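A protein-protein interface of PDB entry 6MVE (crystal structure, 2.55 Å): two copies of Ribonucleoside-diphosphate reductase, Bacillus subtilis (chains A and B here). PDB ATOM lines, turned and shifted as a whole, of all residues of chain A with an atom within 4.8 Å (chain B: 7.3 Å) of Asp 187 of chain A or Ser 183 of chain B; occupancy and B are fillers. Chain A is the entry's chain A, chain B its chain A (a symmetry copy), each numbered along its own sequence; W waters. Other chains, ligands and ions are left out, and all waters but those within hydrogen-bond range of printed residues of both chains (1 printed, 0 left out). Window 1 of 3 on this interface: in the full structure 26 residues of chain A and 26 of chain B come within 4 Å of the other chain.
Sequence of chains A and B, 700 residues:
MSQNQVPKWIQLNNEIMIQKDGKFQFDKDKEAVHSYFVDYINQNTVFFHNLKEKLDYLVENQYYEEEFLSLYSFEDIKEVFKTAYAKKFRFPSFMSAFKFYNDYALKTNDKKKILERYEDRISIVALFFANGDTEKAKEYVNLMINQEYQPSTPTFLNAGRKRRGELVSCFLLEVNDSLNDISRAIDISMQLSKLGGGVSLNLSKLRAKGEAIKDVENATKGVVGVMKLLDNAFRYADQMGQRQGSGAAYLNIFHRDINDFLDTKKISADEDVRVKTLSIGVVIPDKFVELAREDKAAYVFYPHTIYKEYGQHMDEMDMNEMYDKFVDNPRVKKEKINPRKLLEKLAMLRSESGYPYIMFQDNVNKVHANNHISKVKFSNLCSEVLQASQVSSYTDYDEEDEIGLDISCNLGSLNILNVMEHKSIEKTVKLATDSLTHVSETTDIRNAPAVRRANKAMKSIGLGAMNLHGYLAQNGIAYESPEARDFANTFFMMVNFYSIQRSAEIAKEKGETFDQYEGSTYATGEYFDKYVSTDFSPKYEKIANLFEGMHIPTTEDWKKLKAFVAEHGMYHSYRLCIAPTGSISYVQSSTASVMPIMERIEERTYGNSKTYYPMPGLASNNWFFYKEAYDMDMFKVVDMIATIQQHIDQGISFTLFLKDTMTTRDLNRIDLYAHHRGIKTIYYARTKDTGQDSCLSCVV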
ATOM      1  N   SER A 183      25.393  -9.379  29.145  1.00  0.00           N
ATOM      2  CA  SER A 183      24.638 -10.619  28.960  1.00  0.00           C
ATOM      3  C   SER A 183      25.418 -11.817  29.479  1.00  0.00           C
ATOM      4  O   SER A 183      24.838 -12.738  30.062  1.00  0.00           O
ATOM      5  CB  SER A 183      24.293 -10.818  27.490  1.00  0.00           C
ATOM      6  OG  SER A 183      23.427  -9.790  27.081  1.00  0.00           O
ATOM      7  N   ARG A 184      26.732 -11.817  29.279  1.00  0.00           N
ATOM      8  CA  ARG A 184      27.541 -12.938  29.723  1.00  0.00           C
ATOM      9  C   ARG A 184      27.706 -12.949  31.242  1.00  0.00           C
ATOM     10  O   ARG A 184      27.758 -14.026  31.843  1.00  0.00           O
ATOM     11  CB  ARG A 184      28.888 -12.897  28.999  1.00  0.00           C
ATOM     12  CG  ARG A 184      29.916 -13.881  29.490  1.00  0.00           C
ATOM     13  CD  ARG A 184      29.480 -15.273  29.209  1.00  0.00           C
ATOM     14  NE  ARG A 184      29.419 -15.496  27.778  1.00  0.00           N
ATOM     15  CZ  ARG A 184      28.989 -16.621  27.233  1.00  0.00           C
ATOM     16  NH1 ARG A 184      28.583 -17.617  28.020  1.00  0.00           N
ATOM     17  NH2 ARG A 184      28.966 -16.744  25.914  1.00  0.00           N
ATOM     18  N   ALA A 185      27.759 -11.769  31.880  1.00  0.00           N
ATOM     19  CA  ALA A 185      27.823 -11.724  33.340  1.00  0.00           C
ATOM     20  C   ALA A 185      26.521 -12.225  33.957  1.00  0.00           C
ATOM     21  O   ALA A 185      26.539 -12.920  34.979  1.00  0.00           O
ATOM     22  CB  ALA A 185      28.141 -10.307  33.827  1.00  0.00           C
ATOM     23  N   ILE A 186      25.385 -11.902  33.333  1.00  0.00           N
ATOM     24  CA  ILE A 186      24.095 -12.435  33.771  1.00  0.00           C
ATOM     25  C   ILE A 186      24.095 -13.952  33.705  1.00  0.00           C
ATOM     26  O   ILE A 186      23.605 -14.626  34.615  1.00  0.00           O
ATOM     27  CB  ILE A 186      22.943 -11.866  32.921  1.00  0.00           C
ATOM     28  CG1 ILE A 186      22.791 -10.364  33.109  1.00  0.00           C
ATOM     29  CG2 ILE A 186      21.639 -12.564  33.272  1.00  0.00           C
ATOM     30  CD1 ILE A 186      21.812  -9.773  32.090  1.00  0.00           C
ATOM     31  N   ASP A 187      24.628 -14.521  32.624  1.00  0.00           N
ATOM     32  CA  ASP A 187      24.598 -15.974  32.533  1.00  0.00           C
ATOM     33  C   ASP A 187      25.604 -16.615  33.487  1.00  0.00           C
ATOM     34  O   ASP A 187      25.293 -17.628  34.125  1.00  0.00           O
ATOM     35  CB  ASP A 187      24.847 -16.431  31.100  1.00  0.00           C
ATOM     36  CG  ASP A 187      24.933 -17.940  31.001  1.00  0.00           C
ATOM     37  OD1 ASP A 187      24.060 -18.632  31.590  1.00  0.00           O
ATOM     38  OD2 ASP A 187      25.890 -18.439  30.383  1.00  0.00           O
ATOM     39  N   ILE A 188      26.819 -16.064  33.581  1.00  0.00           N
ATOM     40  CA  ILE A 188      27.786 -16.610  34.528  1.00  0.00           C
ATOM     41  C   ILE A 188      27.219 -16.545  35.944  1.00  0.00           C
ATOM     42  O   ILE A 188      27.233 -17.541  36.680  1.00  0.00           O
ATOM     43  CB  ILE A 188      29.132 -15.871  34.425  1.00  0.00           C
ATOM     44  CG1 ILE A 188      29.778 -16.101  33.058  1.00  0.00           C
ATOM     45  CG2 ILE A 188      30.073 -16.337  35.513  1.00  0.00           C
ATOM     46  CD1 ILE A 188      30.853 -15.083  32.703  1.00  0.00           C
ATOM     47  N   SER A 189      26.662 -15.385  36.326  1.00  0.00           N
ATOM     48  CA  SER A 189      26.044 -15.256  37.646  1.00  0.00           C
ATOM     49  C   SER A 189      25.058 -16.390  37.895  1.00  0.00           C
ATOM     50  O   SER A 189      25.064 -17.012  38.966  1.00  0.00           O
ATOM     51  CB  SER A 189      25.341 -13.906  37.786  1.00  0.00           C
ATOM     52  OG  SER A 189      26.268 -12.823  37.778  1.00  0.00           O
ATOM     53  N   MET A 190      24.228 -16.704  36.895  1.00  0.00           N
ATOM     54  CA  MET A 190      23.228 -17.745  37.084  1.00  0.00           C
ATOM     55  C   MET A 190      23.862 -19.129  37.097  1.00  0.00           C
ATOM     56  O   MET A 190      23.393 -20.020  37.814  1.00  0.00           O
ATOM     57  CB  MET A 190      22.149 -17.663  35.999  1.00  0.00           C
ATOM     58  CG  MET A 190      21.193 -16.504  36.161  1.00  0.00           C
ATOM     59  SD  MET A 190      19.689 -16.582  35.164  1.00  0.00           S
ATOM     60  CE  MET A 190      20.326 -16.724  33.492  1.00  0.00           C
ATOM     61  N   GLN A 191      24.904 -19.345  36.287  1.00  0.00           N
ATOM     62  CA  GLN A 191      25.504 -20.676  36.234  1.00  0.00           C
ATOM     63  C   GLN A 191      26.206 -20.995  37.546  1.00  0.00           C
ATOM     64  O   GLN A 191      26.068 -22.101  38.078  1.00  0.00           O
ATOM     65  CB  GLN A 191      26.487 -20.787  35.065  1.00  0.00           C
ATOM     66  CG  GLN A 191      25.896 -20.561  33.676  1.00  0.00           C
ATOM     67  CD  GLN A 191      25.083 -21.730  33.156  1.00  0.00           C
ATOM     68  OE1 GLN A 191      25.245 -22.870  33.586  1.00  0.00           O
ATOM     69  NE2 GLN A 191      24.205 -21.446  32.218  1.00  0.00           N
ATOM     70  N   VAL B 175      12.914 -21.238  22.065  1.00  0.00           N
ATOM     71  CA  VAL B 175      13.708 -21.315  23.292  1.00  0.00           C
ATOM     72  C   VAL B 175      13.704 -22.750  23.791  1.00  0.00           C
ATOM     73  O   VAL B 175      12.643 -23.298  24.111  1.00  0.00           O
ATOM     74  CB  VAL B 175      13.181 -20.375  24.389  1.00  0.00           C
ATOM     75  CG1 VAL B 175      14.166 -20.326  25.539  1.00  0.00           C
ATOM     76  CG2 VAL B 175      12.903 -18.971  23.832  1.00  0.00           C
ATOM     77  N   SER B 178      16.540 -25.333  28.800  1.00  0.00           N
ATOM     78  CA  SER B 178      17.767 -25.373  29.599  1.00  0.00           C
ATOM     79  C   SER B 178      18.163 -23.960  29.999  1.00  0.00           C
ATOM     80  O   SER B 178      17.748 -22.976  29.374  1.00  0.00           O
ATOM     81  CB  SER B 178      18.925 -26.040  28.847  1.00  0.00           C
ATOM     82  OG  SER B 178      19.618 -25.106  28.024  1.00  0.00           O
ATOM     83  N   LEU B 179      18.997 -23.871  31.040  1.00  0.00           N
ATOM     84  CA  LEU B 179      19.471 -22.560  31.480  1.00  0.00           C
ATOM     85  C   LEU B 179      20.338 -21.895  30.411  1.00  0.00           C
ATOM     86  O   LEU B 179      20.207 -20.692  30.157  1.00  0.00           O
ATOM     87  CB  LEU B 179      20.230 -22.692  32.802  1.00  0.00           C
ATOM     88  CG  LEU B 179      20.711 -21.387  33.434  1.00  0.00           C
ATOM     89  CD1 LEU B 179      19.530 -20.492  33.779  1.00  0.00           C
ATOM     90  CD2 LEU B 179      21.563 -21.647  34.647  1.00  0.00           C
ATOM     91  N   ASN B 180      21.220 -22.665  29.765  1.00  0.00           N
ATOM     92  CA  ASN B 180      21.998 -22.144  28.644  1.00  0.00           C
ATOM     93  C   ASN B 180      21.101 -21.466  27.609  1.00  0.00           C
ATOM     94  O   ASN B 180      21.401 -20.362  27.130  1.00  0.00           O
ATOM     95  CB  ASN B 180      22.781 -23.269  27.969  1.00  0.00           C
ATOM     96  CG  ASN B 180      23.817 -23.905  28.865  1.00  0.00           C
ATOM     97  OD1 ASN B 180      24.150 -23.407  29.946  1.00  0.00           O
ATOM     98  ND2 ASN B 180      24.357 -25.017  28.398  1.00  0.00           N
ATOM     99  N   ASP B 181      19.989 -22.118  27.249  1.00  0.00           N
ATOM    100  CA  ASP B 181      19.146 -21.593  26.177  1.00  0.00           C
ATOM    101  C   ASP B 181      18.373 -20.364  26.632  1.00  0.00           C
ATOM    102  O   ASP B 181      18.210 -19.406  25.865  1.00  0.00           O
ATOM    103  CB  ASP B 181      18.203 -22.682  25.667  1.00  0.00           C
ATOM    104  CG  ASP B 181      18.947 -23.790  24.904  1.00  0.00           C
ATOM    105  OD1 ASP B 181      19.445 -23.510  23.789  1.00  0.00           O
ATOM    106  OD2 ASP B 181      19.060 -24.933  25.432  1.00  0.00           O
ATOM    107  N   ILE B 182      17.917 -20.361  27.885  1.00  0.00           N
ATOM    108  CA  ILE B 182      17.241 -19.195  28.438  1.00  0.00           C
ATOM    109  C   ILE B 182      18.178 -17.996  28.463  1.00  0.00           C
ATOM    110  O   ILE B 182      17.782 -16.875  28.116  1.00  0.00           O
ATOM    111  CB  ILE B 182      16.694 -19.517  29.839  1.00  0.00           C
ATOM    112  CG1 ILE B 182      15.570 -20.530  29.726  1.00  0.00           C
ATOM    113  CG2 ILE B 182      16.231 -18.256  30.540  1.00  0.00           C
ATOM    114  CD1 ILE B 182      15.135 -21.070  31.040  1.00  0.00           C
ATOM    115  N   SER B 183      19.432 -18.205  28.876  1.00  0.00           N
ATOM    116  CA  SER B 183      20.381 -17.090  28.893  1.00  0.00           C
ATOM    117  C   SER B 183      20.617 -16.551  27.490  1.00  0.00           C
ATOM    118  O   SER B 183      20.748 -15.339  27.297  1.00  0.00           O
ATOM    119  CB  SER B 183      21.702 -17.525  29.515  1.00  0.00           C
ATOM    120  OG  SER B 183      21.486 -17.850  30.864  1.00  0.00           O
ATOM    121  N   ARG B 184      20.671 -17.438  26.502  1.00  0.00           N
ATOM    122  CA  ARG B 184      20.919 -17.003  25.139  1.00  0.00           C
ATOM    123  C   ARG B 184      19.698 -16.308  24.537  1.00  0.00           C
ATOM    124  O   ARG B 184      19.857 -15.367  23.753  1.00  0.00           O
ATOM    125  CB  ARG B 184      21.363 -18.207  24.305  1.00  0.00           C
ATOM    126  CG  ARG B 184      21.475 -17.962  22.824  1.00  0.00           C
ATOM    127  CD  ARG B 184      22.564 -16.993  22.537  1.00  0.00           C
ATOM    128  NE  ARG B 184      23.845 -17.562  22.907  1.00  0.00           N
ATOM    129  CZ  ARG B 184      24.986 -16.898  22.834  1.00  0.00           C
ATOM    130  NH1 ARG B 184      24.984 -15.638  22.403  1.00  0.00           N
ATOM    131  NH2 ARG B 184      26.114 -17.493  23.193  1.00  0.00           N
ATOM    132  N   ALA B 185      18.481 -16.732  24.911  1.00  0.00           N
ATOM    133  CA  ALA B 185      17.283 -16.041  24.438  1.00  0.00           C
ATOM    134  C   ALA B 185      17.194 -14.638  25.029  1.00  0.00           C
ATOM    135  O   ALA B 185      16.791 -13.694  24.342  1.00  0.00           O
ATOM    136  CB  ALA B 185      16.023 -16.847  24.769  1.00  0.00           C
ATOM    137  N   ILE B 186      17.592 -14.482  26.294  1.00  0.00           N
ATOM    138  CA  ILE B 186      17.665 -13.160  26.915  1.00  0.00           C
ATOM    139  C   ILE B 186      18.622 -12.264  26.149  1.00  0.00           C
ATOM    140  O   ILE B 186      18.337 -11.087  25.913  1.00  0.00           O
ATOM    141  CB  ILE B 186      18.098 -13.263  28.390  1.00  0.00           C
ATOM    142  CG1 ILE B 186      17.065 -13.995  29.232  1.00  0.00           C
ATOM    143  CG2 ILE B 186      18.339 -11.875  28.963  1.00  0.00           C
ATOM    144  CD1 ILE B 186      17.606 -14.302  30.632  1.00  0.00           C
ATOM    145  N   ASP B 187      19.782 -12.792  25.758  1.00  0.00           N
ATOM    146  CA  ASP B 187      20.722 -11.931  25.058  1.00  0.00           C
ATOM    147  C   ASP B 187      20.261 -11.643  23.630  1.00  0.00           C
ATOM    148  O   ASP B 187      20.380 -10.506  23.158  1.00  0.00           O
ATOM    149  CB  ASP B 187      22.119 -12.542  25.060  1.00  0.00           C
ATOM    150  CG  ASP B 187      23.092 -11.719  24.239  1.00  0.00           C
ATOM    151  OD1 ASP B 187      23.104 -10.469  24.398  1.00  0.00           O
ATOM    152  OD2 ASP B 187      23.804 -12.303  23.405  1.00  0.00           O
ATOM    153  N   ILE B 188      19.759 -12.656  22.916  1.00  0.00           N
ATOM    154  CA  ILE B 188      19.249 -12.407  21.571  1.00  0.00           C
ATOM    155  C   ILE B 188      18.126 -11.375  21.625  1.00  0.00           C
ATOM    156  O   ILE B 188      18.130 -10.391  20.873  1.00  0.00           O
ATOM    157  CB  ILE B 188      18.782 -13.716  20.910  1.00  0.00           C
ATOM    158  CG1 ILE B 188      19.959 -14.669  20.693  1.00  0.00           C
ATOM    159  CG2 ILE B 188      18.114 -13.428  19.586  1.00  0.00           C
ATOM    160  CD1 ILE B 188      19.549 -16.118  20.471  1.00  0.00           C
ATOM    161  N   SER B 189      17.174 -11.557  22.555  1.00  0.00           N
ATOM    162  CA  SER B 189      16.093 -10.583  22.712  1.00  0.00           C
ATOM    163  C   SER B 189      16.651  -9.171  22.835  1.00  0.00           C
ATOM    164  O   SER B 189      16.166  -8.238  22.181  1.00  0.00           O
ATOM    165  CB  SER B 189      15.234 -10.920  23.930  1.00  0.00           C
ATOM    166  OG  SER B 189      14.520 -12.141  23.753  1.00  0.00           O
ATOM    167  N   MET B 190      17.704  -9.002  23.641  1.00  0.00           N
ATOM    168  CA  MET B 190      18.255  -7.670  23.843  1.00  0.00           C
ATOM    169  C   MET B 190      19.018  -7.192  22.615  1.00  0.00           C
ATOM    170  O   MET B 190      19.014  -5.994  22.309  1.00  0.00           O
ATOM    171  CB  MET B 190      19.160  -7.639  25.079  1.00  0.00           C
ATOM    172  CG  MET B 190      18.417  -7.696  26.394  1.00  0.00           C
ATOM    173  SD  MET B 190      19.382  -7.268  27.860  1.00  0.00           S
ATOM    174  CE  MET B 190      20.750  -8.428  27.788  1.00  0.00           C
ATOM    175  N   LEU B 229      12.338 -12.582  33.522  1.00  0.00           N
ATOM    176  CA  LEU B 229      13.649 -12.207  33.002  1.00  0.00           C
ATOM    177  C   LEU B 229      13.525 -11.495  31.655  1.00  0.00           C
ATOM    178  O   LEU B 229      14.217 -10.503  31.408  1.00  0.00           O
ATOM    179  CB  LEU B 229      14.550 -13.443  32.893  1.00  0.00           C
ATOM    180  CG  LEU B 229      14.930 -14.193  34.171  1.00  0.00           C
ATOM    181  CD1 LEU B 229      15.555 -15.551  33.849  1.00  0.00           C
ATOM    182  CD2 LEU B 229      15.864 -13.363  35.032  1.00  0.00           C
ATOM    183  N   TYR B 394      21.823 -24.122  22.552  1.00  0.00           N
ATOM    184  CA  TYR B 394      23.042 -23.416  22.895  1.00  0.00           C
ATOM    185  C   TYR B 394      23.643 -24.173  24.064  1.00  0.00           C
ATOM    186  O   TYR B 394      23.070 -24.193  25.156  1.00  0.00           O
ATOM    187  CB  TYR B 394      22.728 -21.958  23.208  1.00  0.00           C
ATOM    188  CG  TYR B 394      22.060 -21.274  22.027  1.00  0.00           C
ATOM    189  CD1 TYR B 394      22.808 -20.831  20.950  1.00  0.00           C
ATOM    190  CD2 TYR B 394      20.672 -21.109  21.975  1.00  0.00           C
ATOM    191  CE1 TYR B 394      22.198 -20.210  19.849  1.00  0.00           C
ATOM    192  CE2 TYR B 394      20.059 -20.496  20.895  1.00  0.00           C
ATOM    193  CZ  TYR B 394      20.825 -20.051  19.828  1.00  0.00           C
ATOM    194  OH  TYR B 394      20.227 -19.450  18.740  1.00  0.00           O
ATOM    195  N   THR B 395      24.745 -24.864  23.810  1.00  0.00           N
ATOM    196  CA  THR B 395      25.345 -25.775  24.770  1.00  0.00           C
ATOM    197  C   THR B 395      26.325 -25.018  25.660  1.00  0.00           C
ATOM    198  O   THR B 395      26.464 -23.793  25.577  1.00  0.00           O
ATOM    199  CB  THR B 395      26.046 -26.919  24.047  1.00  0.00           C
ATOM    200  OG1 THR B 395      27.024 -26.368  23.157  1.00  0.00           O
ATOM    201  CG2 THR B 395      25.059 -27.737  23.270  1.00  0.00           C
ATOM    202  N   TYR B 397      29.790 -23.501  27.309  1.00  0.00           N
ATOM    203  CA  TYR B 397      30.667 -22.526  26.674  1.00  0.00           C
ATOM    204  C   TYR B 397      31.748 -23.193  25.833  1.00  0.00           C
ATOM    205  O   TYR B 397      32.098 -22.698  24.756  1.00  0.00           O
ATOM    206  CB  TYR B 397      31.291 -21.626  27.740  1.00  0.00           C
ATOM    207  CG  TYR B 397      32.181 -20.563  27.168  1.00  0.00           C
ATOM    208  CD1 TYR B 397      33.568 -20.718  27.134  1.00  0.00           C
ATOM    209  CD2 TYR B 397      31.639 -19.410  26.639  1.00  0.00           C
ATOM    210  CE1 TYR B 397      34.388 -19.743  26.580  1.00  0.00           C
ATOM    211  CE2 TYR B 397      32.453 -18.422  26.080  1.00  0.00           C
ATOM    212  CZ  TYR B 397      33.822 -18.601  26.052  1.00  0.00           C
ATOM    213  OH  TYR B 397      34.609 -17.619  25.511  1.00  0.00           O
HETATM  214  O   HOH W   1      24.025 -25.142  32.558  1.00  0.00           O
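The side-chain amide nitrogen of Gln 191 of chain A lies within hydrogen-bond range of the side-chain amide oxygen of Asn 180 of chain B (3.0 Å). The side-chain carboxylate (OD1) of Asp 187 of chain B sits at hydrogen-bond distance from the side-chain hydroxyl (OG) of Ser 183 of chain A (2.8 Å). OG of Ser 183 of chain B lies within hydrogen-bond range of OD1 of Asp 187 of chain A (2.8 Å).
The side-chain hydroxyl of Ser 178 of chain B sits close to the backbone NH of Asn 180 of chain B, at 3.4 Å. The side-chain amide nitrogen (NE2) of Gln 191 of chain A is in hydrogen-bond range of the side-chain carboxylate (OD1) of Asp 187 of chain A. The guanidinium group of Arg 184 of chain B is in salt-bridge range of the side-chain carboxylate of Asp 187 of chain B, at 3.7 Å. O of Leu 179 of chain B is in hydrogen-bond range of OG of Ser 183 of chain B. The guanidinium group (NH1) of Arg 184 of chain A lies within salt-bridge range of the side-chain carboxylate (OD2) of Asp 187 of chain A.
Among the printed residues, merely in contact across the chains: Met 190 of chain A with Ser 183 of chain B, Ser 183 of chain A with Met 190 of chain B, Gln 191 of chain A with Leu 179 of chain B, Arg 184 of chain A with Tyr 397 of chain B and Met 190 of chain A with Leu 179 of chain B.
Ser 183 of chain B touches just these residues of chain A: Asp 187 (2.8 Å) and Met 190 (3.1 Å). Of the printed residues of chain B, Ser 183 of chain A touches Asp 187 (2.8 Å) and Met 190 (3.1 Å). Of the printed residues of chain B, Gln 191 of chain A touches Leu 179 and Asn 180. Printed residues of chain A within 4 Å of Asn 180 of chain B: Gln 191. Val 175 of chain B touches none of the printed residues of chain A. Ile 182 of chain B touches none of the printed residues of chain A. The nearest printed residue of chain A that does not touch Tyr 397 of chain B is Asp 187 of chain A (6.8 Å).
Hydrophobic or aromatic side chains of chain A within 4 Å of the printed part of chain B: Met 190. Printed residues of chain B that touch a printed residue of chain A: Leu 179, Asn 180, Ser 183, Asp 187, Met 190 and Tyr 397. Hydrophobic or aromatic side chains of chain B that line the printed part of chain A: Leu 179, Met 190 and Tyr 397. Among the printed residues, no Asp or Glu carboxylate lies within 4 Å of a Lys or Arg side-chain nitrogen of the other chain.
Ser 183 of chain A touches Asp 187 of chain B, and with the chains exchanged Asp 187 of chain A touches Ser 183 of chain B. Ser 183 of chain A touches Met 190 of chain B, and with the chains exchanged Met 190 of chain A touches Ser 183 of chain B. Positions printed for both chains: 183, 184, 185, 186, 187, 188, 189 and 190.
Water W1 bridges OE1 of Gln 191 of chain A (2.8 Å) and OD1 of Asn 180 of chain B (3.1 Å).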
